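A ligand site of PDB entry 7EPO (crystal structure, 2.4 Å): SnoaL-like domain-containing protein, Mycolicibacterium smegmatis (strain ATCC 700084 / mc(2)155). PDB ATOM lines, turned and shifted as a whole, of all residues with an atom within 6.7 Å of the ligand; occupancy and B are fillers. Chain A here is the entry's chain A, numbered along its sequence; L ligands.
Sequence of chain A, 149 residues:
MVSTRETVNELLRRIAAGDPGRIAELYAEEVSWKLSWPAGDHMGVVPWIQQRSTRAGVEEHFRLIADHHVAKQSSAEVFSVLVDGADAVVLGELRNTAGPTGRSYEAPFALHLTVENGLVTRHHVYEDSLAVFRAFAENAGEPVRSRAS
The indole nitrogen (NE1) of Trp 48 lies within hydrogen-bond range of an oxygen (O3) of the ligand (2.8 Å).
An oxygen (O3) of the ligand sits close to the side-chain carboxylate (OE2) of Glu 127 (2.7 Å).
An oxygen (O1) of the ligand is in hydrogen-bond range of a ring nitrogen (NE2) of His 123 (2.7 Å).
O of Leu 94 sits at hydrogen-bond distance from N of Ala 107 (2.7 Å).
The indole nitrogen of Trp 37 is in hydrogen-bond range of the side-chain carboxylate of Glu 127 (2.7 Å).
OH of Tyr 27 lies within hydrogen-bond range of ND1 of His 123 (2.8 Å).
CE1 of His 61 touches O2 of the ligand, at 3.2 Å.
Leu 94 touches the ligand (CG to C4, 3.7 Å).
Val 125 touches the ligand (CG2 to O1, 3.2 Å).
Along chain A the residues within 4 Å of the ligand span positions 48 to 127.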
ATOM      1  N   ILE A  15      28.833 -29.852 -38.909  1.00  0.00           N
ATOM      2  CA  ILE A  15      28.825 -29.648 -37.468  1.00  0.00           C
ATOM      3  C   ILE A  15      28.290 -30.887 -36.769  1.00  0.00           C
ATOM      4  O   ILE A  15      28.877 -31.391 -35.807  1.00  0.00           O
ATOM      5  CB  ILE A  15      28.023 -28.395 -37.089  1.00  0.00           C
ATOM      6  CG1 ILE A  15      28.835 -27.138 -37.406  1.00  0.00           C
ATOM      7  CG2 ILE A  15      27.629 -28.450 -35.626  1.00  0.00           C
ATOM      8  CD1 ILE A  15      28.088 -25.849 -37.155  1.00  0.00           C
ATOM      9  N   TYR A  27      34.685 -21.873 -43.426  1.00  0.00           N
ATOM     10  CA  TYR A  27      34.683 -20.524 -42.907  1.00  0.00           C
ATOM     11  C   TYR A  27      35.698 -19.673 -43.658  1.00  0.00           C
ATOM     12  O   TYR A  27      36.734 -20.169 -44.113  1.00  0.00           O
ATOM     13  CB  TYR A  27      34.996 -20.531 -41.406  1.00  0.00           C
ATOM     14  CG  TYR A  27      33.773 -20.825 -40.578  1.00  0.00           C
ATOM     15  CD1 TYR A  27      33.337 -22.142 -40.375  1.00  0.00           C
ATOM     16  CD2 TYR A  27      33.015 -19.802 -40.033  1.00  0.00           C
ATOM     17  CE1 TYR A  27      32.200 -22.414 -39.632  1.00  0.00           C
ATOM     18  CE2 TYR A  27      31.882 -20.061 -39.290  1.00  0.00           C
ATOM     19  CZ  TYR A  27      31.484 -21.365 -39.097  1.00  0.00           C
ATOM     20  OH  TYR A  27      30.357 -21.596 -38.354  1.00  0.00           O
ATOM     21  N   TRP A  33      32.789 -12.839 -35.466  1.00  0.00           N
ATOM     22  CA  TRP A  33      32.339 -13.844 -34.501  1.00  0.00           C
ATOM     23  C   TRP A  33      31.727 -13.137 -33.302  1.00  0.00           C
ATOM     24  O   TRP A  33      32.413 -12.399 -32.579  1.00  0.00           O
ATOM     25  CB  TRP A  33      33.524 -14.739 -34.110  1.00  0.00           C
ATOM     26  CG  TRP A  33      33.221 -15.814 -33.125  1.00  0.00           C
ATOM     27  CD1 TRP A  33      33.251 -15.715 -31.761  1.00  0.00           C
ATOM     28  CD2 TRP A  33      32.890 -17.182 -33.419  1.00  0.00           C
ATOM     29  NE1 TRP A  33      32.929 -16.919 -31.191  1.00  0.00           N
ATOM     30  CE2 TRP A  33      32.719 -17.838 -32.185  1.00  0.00           C
ATOM     31  CE3 TRP A  33      32.717 -17.911 -34.603  1.00  0.00           C
ATOM     32  CZ2 TRP A  33      32.378 -19.194 -32.092  1.00  0.00           C
ATOM     33  CZ3 TRP A  33      32.372 -19.259 -34.509  1.00  0.00           C
ATOM     34  CH2 TRP A  33      32.209 -19.888 -33.265  1.00  0.00           C
ATOM     35  N   LEU A  35      28.702 -13.353 -29.909  1.00  0.00           N
ATOM     36  CA  LEU A  35      27.956 -14.204 -29.003  1.00  0.00           C
ATOM     37  C   LEU A  35      27.138 -13.333 -28.064  1.00  0.00           C
ATOM     38  O   LEU A  35      27.627 -12.295 -27.597  1.00  0.00           O
ATOM     39  CB  LEU A  35      28.907 -15.108 -28.206  1.00  0.00           C
ATOM     40  CG  LEU A  35      29.982 -15.868 -28.994  1.00  0.00           C
ATOM     41  CD1 LEU A  35      31.000 -16.522 -28.061  1.00  0.00           C
ATOM     42  CD2 LEU A  35      29.358 -16.930 -29.922  1.00  0.00           C
ATOM     43  N   TRP A  37      26.609 -13.115 -24.999  1.00  0.00           N
ATOM     44  CA  TRP A  37      27.185 -13.273 -23.668  1.00  0.00           C
ATOM     45  C   TRP A  37      27.838 -11.962 -23.256  1.00  0.00           C
ATOM     46  O   TRP A  37      28.321 -11.208 -24.104  1.00  0.00           O
ATOM     47  CB  TRP A  37      28.250 -14.389 -23.657  1.00  0.00           C
ATOM     48  CG  TRP A  37      27.663 -15.708 -23.776  1.00  0.00           C
ATOM     49  CD1 TRP A  37      27.005 -16.215 -24.861  1.00  0.00           C
ATOM     50  CD2 TRP A  37      27.640 -16.724 -22.782  1.00  0.00           C
ATOM     51  NE1 TRP A  37      26.595 -17.493 -24.602  1.00  0.00           N
ATOM     52  CE2 TRP A  37      26.959 -17.836 -23.335  1.00  0.00           C
ATOM     53  CE3 TRP A  37      28.150 -16.810 -21.483  1.00  0.00           C
ATOM     54  CZ2 TRP A  37      26.771 -19.010 -22.634  1.00  0.00           C
ATOM     55  CZ3 TRP A  37      27.949 -17.980 -20.778  1.00  0.00           C
ATOM     56  CH2 TRP A  37      27.271 -19.072 -21.362  1.00  0.00           C
ATOM     57  N   VAL A  46      32.210 -20.567 -18.465  1.00  0.00           N
ATOM     58  CA  VAL A  46      31.821 -21.284 -19.704  1.00  0.00           C
ATOM     59  C   VAL A  46      32.930 -21.056 -20.722  1.00  0.00           C
ATOM     60  O   VAL A  46      33.120 -19.936 -21.207  1.00  0.00           O
ATOM     61  CB  VAL A  46      30.473 -20.754 -20.231  1.00  0.00           C
ATOM     62  CG1 VAL A  46      30.070 -21.512 -21.488  1.00  0.00           C
ATOM     63  CG2 VAL A  46      29.403 -20.910 -19.159  1.00  0.00           C
ATOM     64  N   TRP A  48      34.096 -21.859 -23.919  1.00  0.00           N
ATOM     65  CA  TRP A  48      34.155 -21.450 -25.319  1.00  0.00           C
ATOM     66  C   TRP A  48      33.794 -19.985 -25.508  1.00  0.00           C
ATOM     67  O   TRP A  48      34.160 -19.397 -26.528  1.00  0.00           O
ATOM     68  CB  TRP A  48      33.271 -22.348 -26.182  1.00  0.00           C
ATOM     69  CG  TRP A  48      31.866 -22.486 -25.734  1.00  0.00           C
ATOM     70  CD1 TRP A  48      30.785 -21.798 -26.192  1.00  0.00           C
ATOM     71  CD2 TRP A  48      31.371 -23.393 -24.742  1.00  0.00           C
ATOM     72  NE1 TRP A  48      29.650 -22.204 -25.547  1.00  0.00           N
ATOM     73  CE2 TRP A  48      29.977 -23.179 -24.657  1.00  0.00           C
ATOM     74  CE3 TRP A  48      31.953 -24.356 -23.921  1.00  0.00           C
ATOM     75  CZ2 TRP A  48      29.168 -23.908 -23.781  1.00  0.00           C
ATOM     76  CZ3 TRP A  48      31.153 -25.066 -23.057  1.00  0.00           C
ATOM     77  CH2 TRP A  48      29.770 -24.840 -22.995  1.00  0.00           C
ATOM     78  N   ILE A  49      33.119 -19.377 -24.534  1.00  0.00           N
ATOM     79  CA  ILE A  49      32.720 -17.989 -24.633  1.00  0.00           C
ATOM     80  C   ILE A  49      33.963 -17.100 -24.656  1.00  0.00           C
ATOM     81  O   ILE A  49      34.514 -16.744 -23.610  1.00  0.00           O
ATOM     82  CB  ILE A  49      31.781 -17.614 -23.462  1.00  0.00           C
ATOM     83  CG1 ILE A  49      30.611 -18.598 -23.390  1.00  0.00           C
ATOM     84  CG2 ILE A  49      31.301 -16.163 -23.577  1.00  0.00           C
ATOM     85  CD1 ILE A  49      29.839 -18.764 -24.690  1.00  0.00           C
ATOM     86  N   HIS A  61      37.340 -23.344 -31.626  1.00  0.00           N
ATOM     87  CA  HIS A  61      36.038 -23.319 -30.971  1.00  0.00           C
ATOM     88  C   HIS A  61      35.362 -24.675 -31.057  1.00  0.00           C
ATOM     89  O   HIS A  61      34.854 -25.202 -30.058  1.00  0.00           O
ATOM     90  CB  HIS A  61      35.162 -22.262 -31.606  1.00  0.00           C
ATOM     91  CG  HIS A  61      33.714 -22.406 -31.250  1.00  0.00           C
ATOM     92  ND1 HIS A  61      32.752 -22.788 -32.154  1.00  0.00           N
ATOM     93  CD2 HIS A  61      33.075 -22.245 -30.065  1.00  0.00           C
ATOM     94  CE1 HIS A  61      31.579 -22.830 -31.548  1.00  0.00           C
ATOM     95  NE2 HIS A  61      31.748 -22.497 -30.285  1.00  0.00           N
ATOM     96  N   PHE A  62      35.338 -25.265 -32.255  1.00  0.00           N
ATOM     97  CA  PHE A  62      34.662 -26.536 -32.411  1.00  0.00           C
ATOM     98  C   PHE A  62      35.429 -27.668 -31.728  1.00  0.00           C
ATOM     99  O   PHE A  62      34.822 -28.650 -31.290  1.00  0.00           O
ATOM    100  CB  PHE A  62      34.408 -26.818 -33.887  1.00  0.00           C
ATOM    101  CG  PHE A  62      33.308 -25.962 -34.479  1.00  0.00           C
ATOM    102  CD1 PHE A  62      31.975 -26.252 -34.232  1.00  0.00           C
ATOM    103  CD2 PHE A  62      33.613 -24.854 -35.266  1.00  0.00           C
ATOM    104  CE1 PHE A  62      30.955 -25.456 -34.755  1.00  0.00           C
ATOM    105  CE2 PHE A  62      32.607 -24.062 -35.792  1.00  0.00           C
ATOM    106  CZ  PHE A  62      31.273 -24.366 -35.536  1.00  0.00           C
ATOM    107  N   ILE A  65      34.075 -26.910 -27.683  1.00  0.00           N
ATOM    108  CA  ILE A  65      32.743 -27.371 -27.288  1.00  0.00           C
ATOM    109  C   ILE A  65      32.696 -28.897 -27.240  1.00  0.00           C
ATOM    110  O   ILE A  65      31.963 -29.485 -26.431  1.00  0.00           O
ATOM    111  CB  ILE A  65      31.650 -26.808 -28.225  1.00  0.00           C
ATOM    112  CG1 ILE A  65      32.017 -27.007 -29.679  1.00  0.00           C
ATOM    113  CG2 ILE A  65      31.316 -25.344 -27.912  1.00  0.00           C
ATOM    114  CD1 ILE A  65      32.107 -28.424 -30.069  1.00  0.00           C
ATOM    115  N   LEU A  94      20.015 -26.279 -28.264  1.00  0.00           N
ATOM    116  CA  LEU A  94      21.104 -27.076 -27.709  1.00  0.00           C
ATOM    117  C   LEU A  94      20.598 -27.815 -26.470  1.00  0.00           C
ATOM    118  O   LEU A  94      20.097 -27.190 -25.532  1.00  0.00           O
ATOM    119  CB  LEU A  94      22.273 -26.188 -27.297  1.00  0.00           C
ATOM    120  CG  LEU A  94      23.509 -26.065 -28.177  1.00  0.00           C
ATOM    121  CD1 LEU A  94      24.401 -27.282 -27.999  1.00  0.00           C
ATOM    122  CD2 LEU A  94      23.089 -25.888 -29.612  1.00  0.00           C
ATOM    123  N   ASN A  96      22.608 -30.226 -24.245  1.00  0.00           N
ATOM    124  CA  ASN A  96      23.867 -30.870 -23.885  1.00  0.00           C
ATOM    125  C   ASN A  96      23.940 -31.024 -22.366  1.00  0.00           C
ATOM    126  O   ASN A  96      22.982 -30.772 -21.640  1.00  0.00           O
ATOM    127  CB  ASN A  96      25.062 -30.054 -24.395  1.00  0.00           C
ATOM    128  CG  ASN A  96      25.183 -30.083 -25.902  1.00  0.00           C
ATOM    129  OD1 ASN A  96      24.204 -30.252 -26.617  1.00  0.00           O
ATOM    130  ND2 ASN A  96      26.404 -29.882 -26.391  1.00  0.00           N
ATOM    131  N   TYR A 105      21.556 -29.230 -19.484  1.00  0.00           N
ATOM    132  CA  TYR A 105      20.952 -27.945 -19.800  1.00  0.00           C
ATOM    133  C   TYR A 105      20.362 -27.945 -21.206  1.00  0.00           C
ATOM    134  O   TYR A 105      20.731 -28.733 -22.072  1.00  0.00           O
ATOM    135  CB  TYR A 105      21.963 -26.780 -19.646  1.00  0.00           C
ATOM    136  CG  TYR A 105      23.008 -26.670 -20.744  1.00  0.00           C
ATOM    137  CD1 TYR A 105      22.733 -25.996 -21.919  1.00  0.00           C
ATOM    138  CD2 TYR A 105      24.273 -27.233 -20.590  1.00  0.00           C
ATOM    139  CE1 TYR A 105      23.680 -25.890 -22.929  1.00  0.00           C
ATOM    140  CE2 TYR A 105      25.226 -27.128 -21.581  1.00  0.00           C
ATOM    141  CZ  TYR A 105      24.921 -26.462 -22.748  1.00  0.00           C
ATOM    142  OH  TYR A 105      25.855 -26.353 -23.754  1.00  0.00           O
ATOM    143  N   ALA A 107      19.495 -24.942 -24.153  1.00  0.00           N
ATOM    144  CA  ALA A 107      19.616 -23.550 -24.548  1.00  0.00           C
ATOM    145  C   ALA A 107      19.009 -23.364 -25.931  1.00  0.00           C
ATOM    146  O   ALA A 107      19.558 -23.914 -26.920  1.00  0.00           O
ATOM    147  CB  ALA A 107      21.071 -23.086 -24.531  1.00  0.00           C
ATOM    148  N   PHE A 109      18.656 -21.450 -29.350  1.00  0.00           N
ATOM    149  CA  PHE A 109      19.594 -20.594 -30.059  1.00  0.00           C
ATOM    150  C   PHE A 109      18.999 -20.141 -31.384  1.00  0.00           C
ATOM    151  O   PHE A 109      18.185 -20.832 -32.009  1.00  0.00           O
ATOM    152  CB  PHE A 109      20.936 -21.301 -30.315  1.00  0.00           C
ATOM    153  CG  PHE A 109      20.867 -22.385 -31.364  1.00  0.00           C
ATOM    154  CD1 PHE A 109      21.013 -22.088 -32.709  1.00  0.00           C
ATOM    155  CD2 PHE A 109      20.644 -23.704 -30.991  1.00  0.00           C
ATOM    156  CE1 PHE A 109      20.931 -23.080 -33.668  1.00  0.00           C
ATOM    157  CE2 PHE A 109      20.581 -24.707 -31.956  1.00  0.00           C
ATOM    158  CZ  PHE A 109      20.716 -24.393 -33.297  1.00  0.00           C
ATOM    159  N   LEU A 111      21.128 -18.854 -34.711  1.00  0.00           N
ATOM    160  CA  LEU A 111      22.493 -18.745 -35.253  1.00  0.00           C
ATOM    161  C   LEU A 111      22.430 -17.913 -36.532  1.00  0.00           C
ATOM    162  O   LEU A 111      21.855 -18.349 -37.543  1.00  0.00           O
ATOM    163  CB  LEU A 111      23.087 -20.122 -35.519  1.00  0.00           C
ATOM    164  CG  LEU A 111      24.432 -20.209 -36.208  1.00  0.00           C
ATOM    165  CD1 LEU A 111      25.490 -19.461 -35.430  1.00  0.00           C
ATOM    166  CD2 LEU A 111      24.841 -21.642 -36.332  1.00  0.00           C
ATOM    167  N   HIS A 123      29.365 -15.342 -38.013  1.00  0.00           N
ATOM    168  CA  HIS A 123      28.816 -16.378 -37.136  1.00  0.00           C
ATOM    169  C   HIS A 123      28.463 -15.684 -35.811  1.00  0.00           C
ATOM    170  O   HIS A 123      29.342 -15.380 -35.001  1.00  0.00           O
ATOM    171  CB  HIS A 123      29.831 -17.499 -36.946  1.00  0.00           C
ATOM    172  CG  HIS A 123      29.399 -18.604 -36.021  1.00  0.00           C
ATOM    173  ND1 HIS A 123      29.263 -19.912 -36.449  1.00  0.00           N
ATOM    174  CD2 HIS A 123      29.152 -18.617 -34.690  1.00  0.00           C
ATOM    175  CE1 HIS A 123      28.926 -20.673 -35.422  1.00  0.00           C
ATOM    176  NE2 HIS A 123      28.844 -19.909 -34.344  1.00  0.00           N
ATOM    177  N   VAL A 125      25.992 -15.923 -32.600  1.00  0.00           N
ATOM    178  CA  VAL A 125      25.077 -16.783 -31.856  1.00  0.00           C
ATOM    179  C   VAL A 125      24.245 -15.930 -30.924  1.00  0.00           C
ATOM    180  O   VAL A 125      24.785 -15.079 -30.199  1.00  0.00           O
ATOM    181  CB  VAL A 125      25.851 -17.849 -31.070  1.00  0.00           C
ATOM    182  CG1 VAL A 125      24.913 -18.590 -30.108  1.00  0.00           C
ATOM    183  CG2 VAL A 125      26.543 -18.808 -32.009  1.00  0.00           C
ATOM    184  N   GLU A 127      21.626 -16.886 -27.876  1.00  0.00           N
ATOM    185  CA  GLU A 127      21.231 -18.084 -27.141  1.00  0.00           C
ATOM    186  C   GLU A 127      21.023 -17.797 -25.654  1.00  0.00           C
ATOM    187  O   GLU A 127      21.509 -16.799 -25.115  1.00  0.00           O
ATOM    188  CB  GLU A 127      22.273 -19.184 -27.279  1.00  0.00           C
ATOM    189  CG  GLU A 127      23.409 -19.072 -26.276  1.00  0.00           C
ATOM    190  CD  GLU A 127      24.645 -19.854 -26.714  1.00  0.00           C
ATOM    191  OE1 GLU A 127      24.472 -20.897 -27.391  1.00  0.00           O
ATOM    192  OE2 GLU A 127      25.769 -19.415 -26.380  1.00  0.00           O
ATOM    193  N   VAL A 132      22.965 -21.873 -19.980  1.00  0.00           N
ATOM    194  CA  VAL A 132      24.301 -22.438 -20.135  1.00  0.00           C
ATOM    195  C   VAL A 132      25.151 -22.081 -18.911  1.00  0.00           C
ATOM    196  O   VAL A 132      25.804 -22.936 -18.302  1.00  0.00           O
ATOM    197  CB  VAL A 132      24.949 -21.922 -21.432  1.00  0.00           C
ATOM    198  CG1 VAL A 132      26.353 -22.481 -21.595  1.00  0.00           C
ATOM    199  CG2 VAL A 132      24.064 -22.249 -22.677  1.00  0.00           C
HETATM  200  O1  LIG L   1      27.878 -21.696 -32.492  1.00  0.00           O
HETATM  201  N1  LIG L   1      28.074 -22.542 -31.696  1.00  0.00           N
HETATM  202  O2  LIG L   1      28.533 -23.570 -32.036  1.00  0.00           O
HETATM  203  C1  LIG L   1      27.790 -22.341 -30.295  1.00  0.00           C
HETATM  204  C2  LIG L   1      27.098 -23.273 -29.531  1.00  0.00           C
HETATM  205  C3  LIG L   1      26.862 -23.026 -28.161  1.00  0.00           C
HETATM  206  C4  LIG L   1      26.219 -23.762 -27.175  1.00  0.00           C
HETATM  207  N2  LIG L   1      26.275 -23.072 -26.024  1.00  0.00           N
HETATM  208  O3  LIG L   1      26.966 -21.887 -26.280  1.00  0.00           O
HETATM  209  C5  LIG L   1      27.318 -21.876 -27.588  1.00  0.00           C
HETATM  210  C6  LIG L   1      28.016 -20.938 -28.364  1.00  0.00           C
HETATM  211  C7  LIG L   1      28.252 -21.177 -29.712  1.00  0.00           C
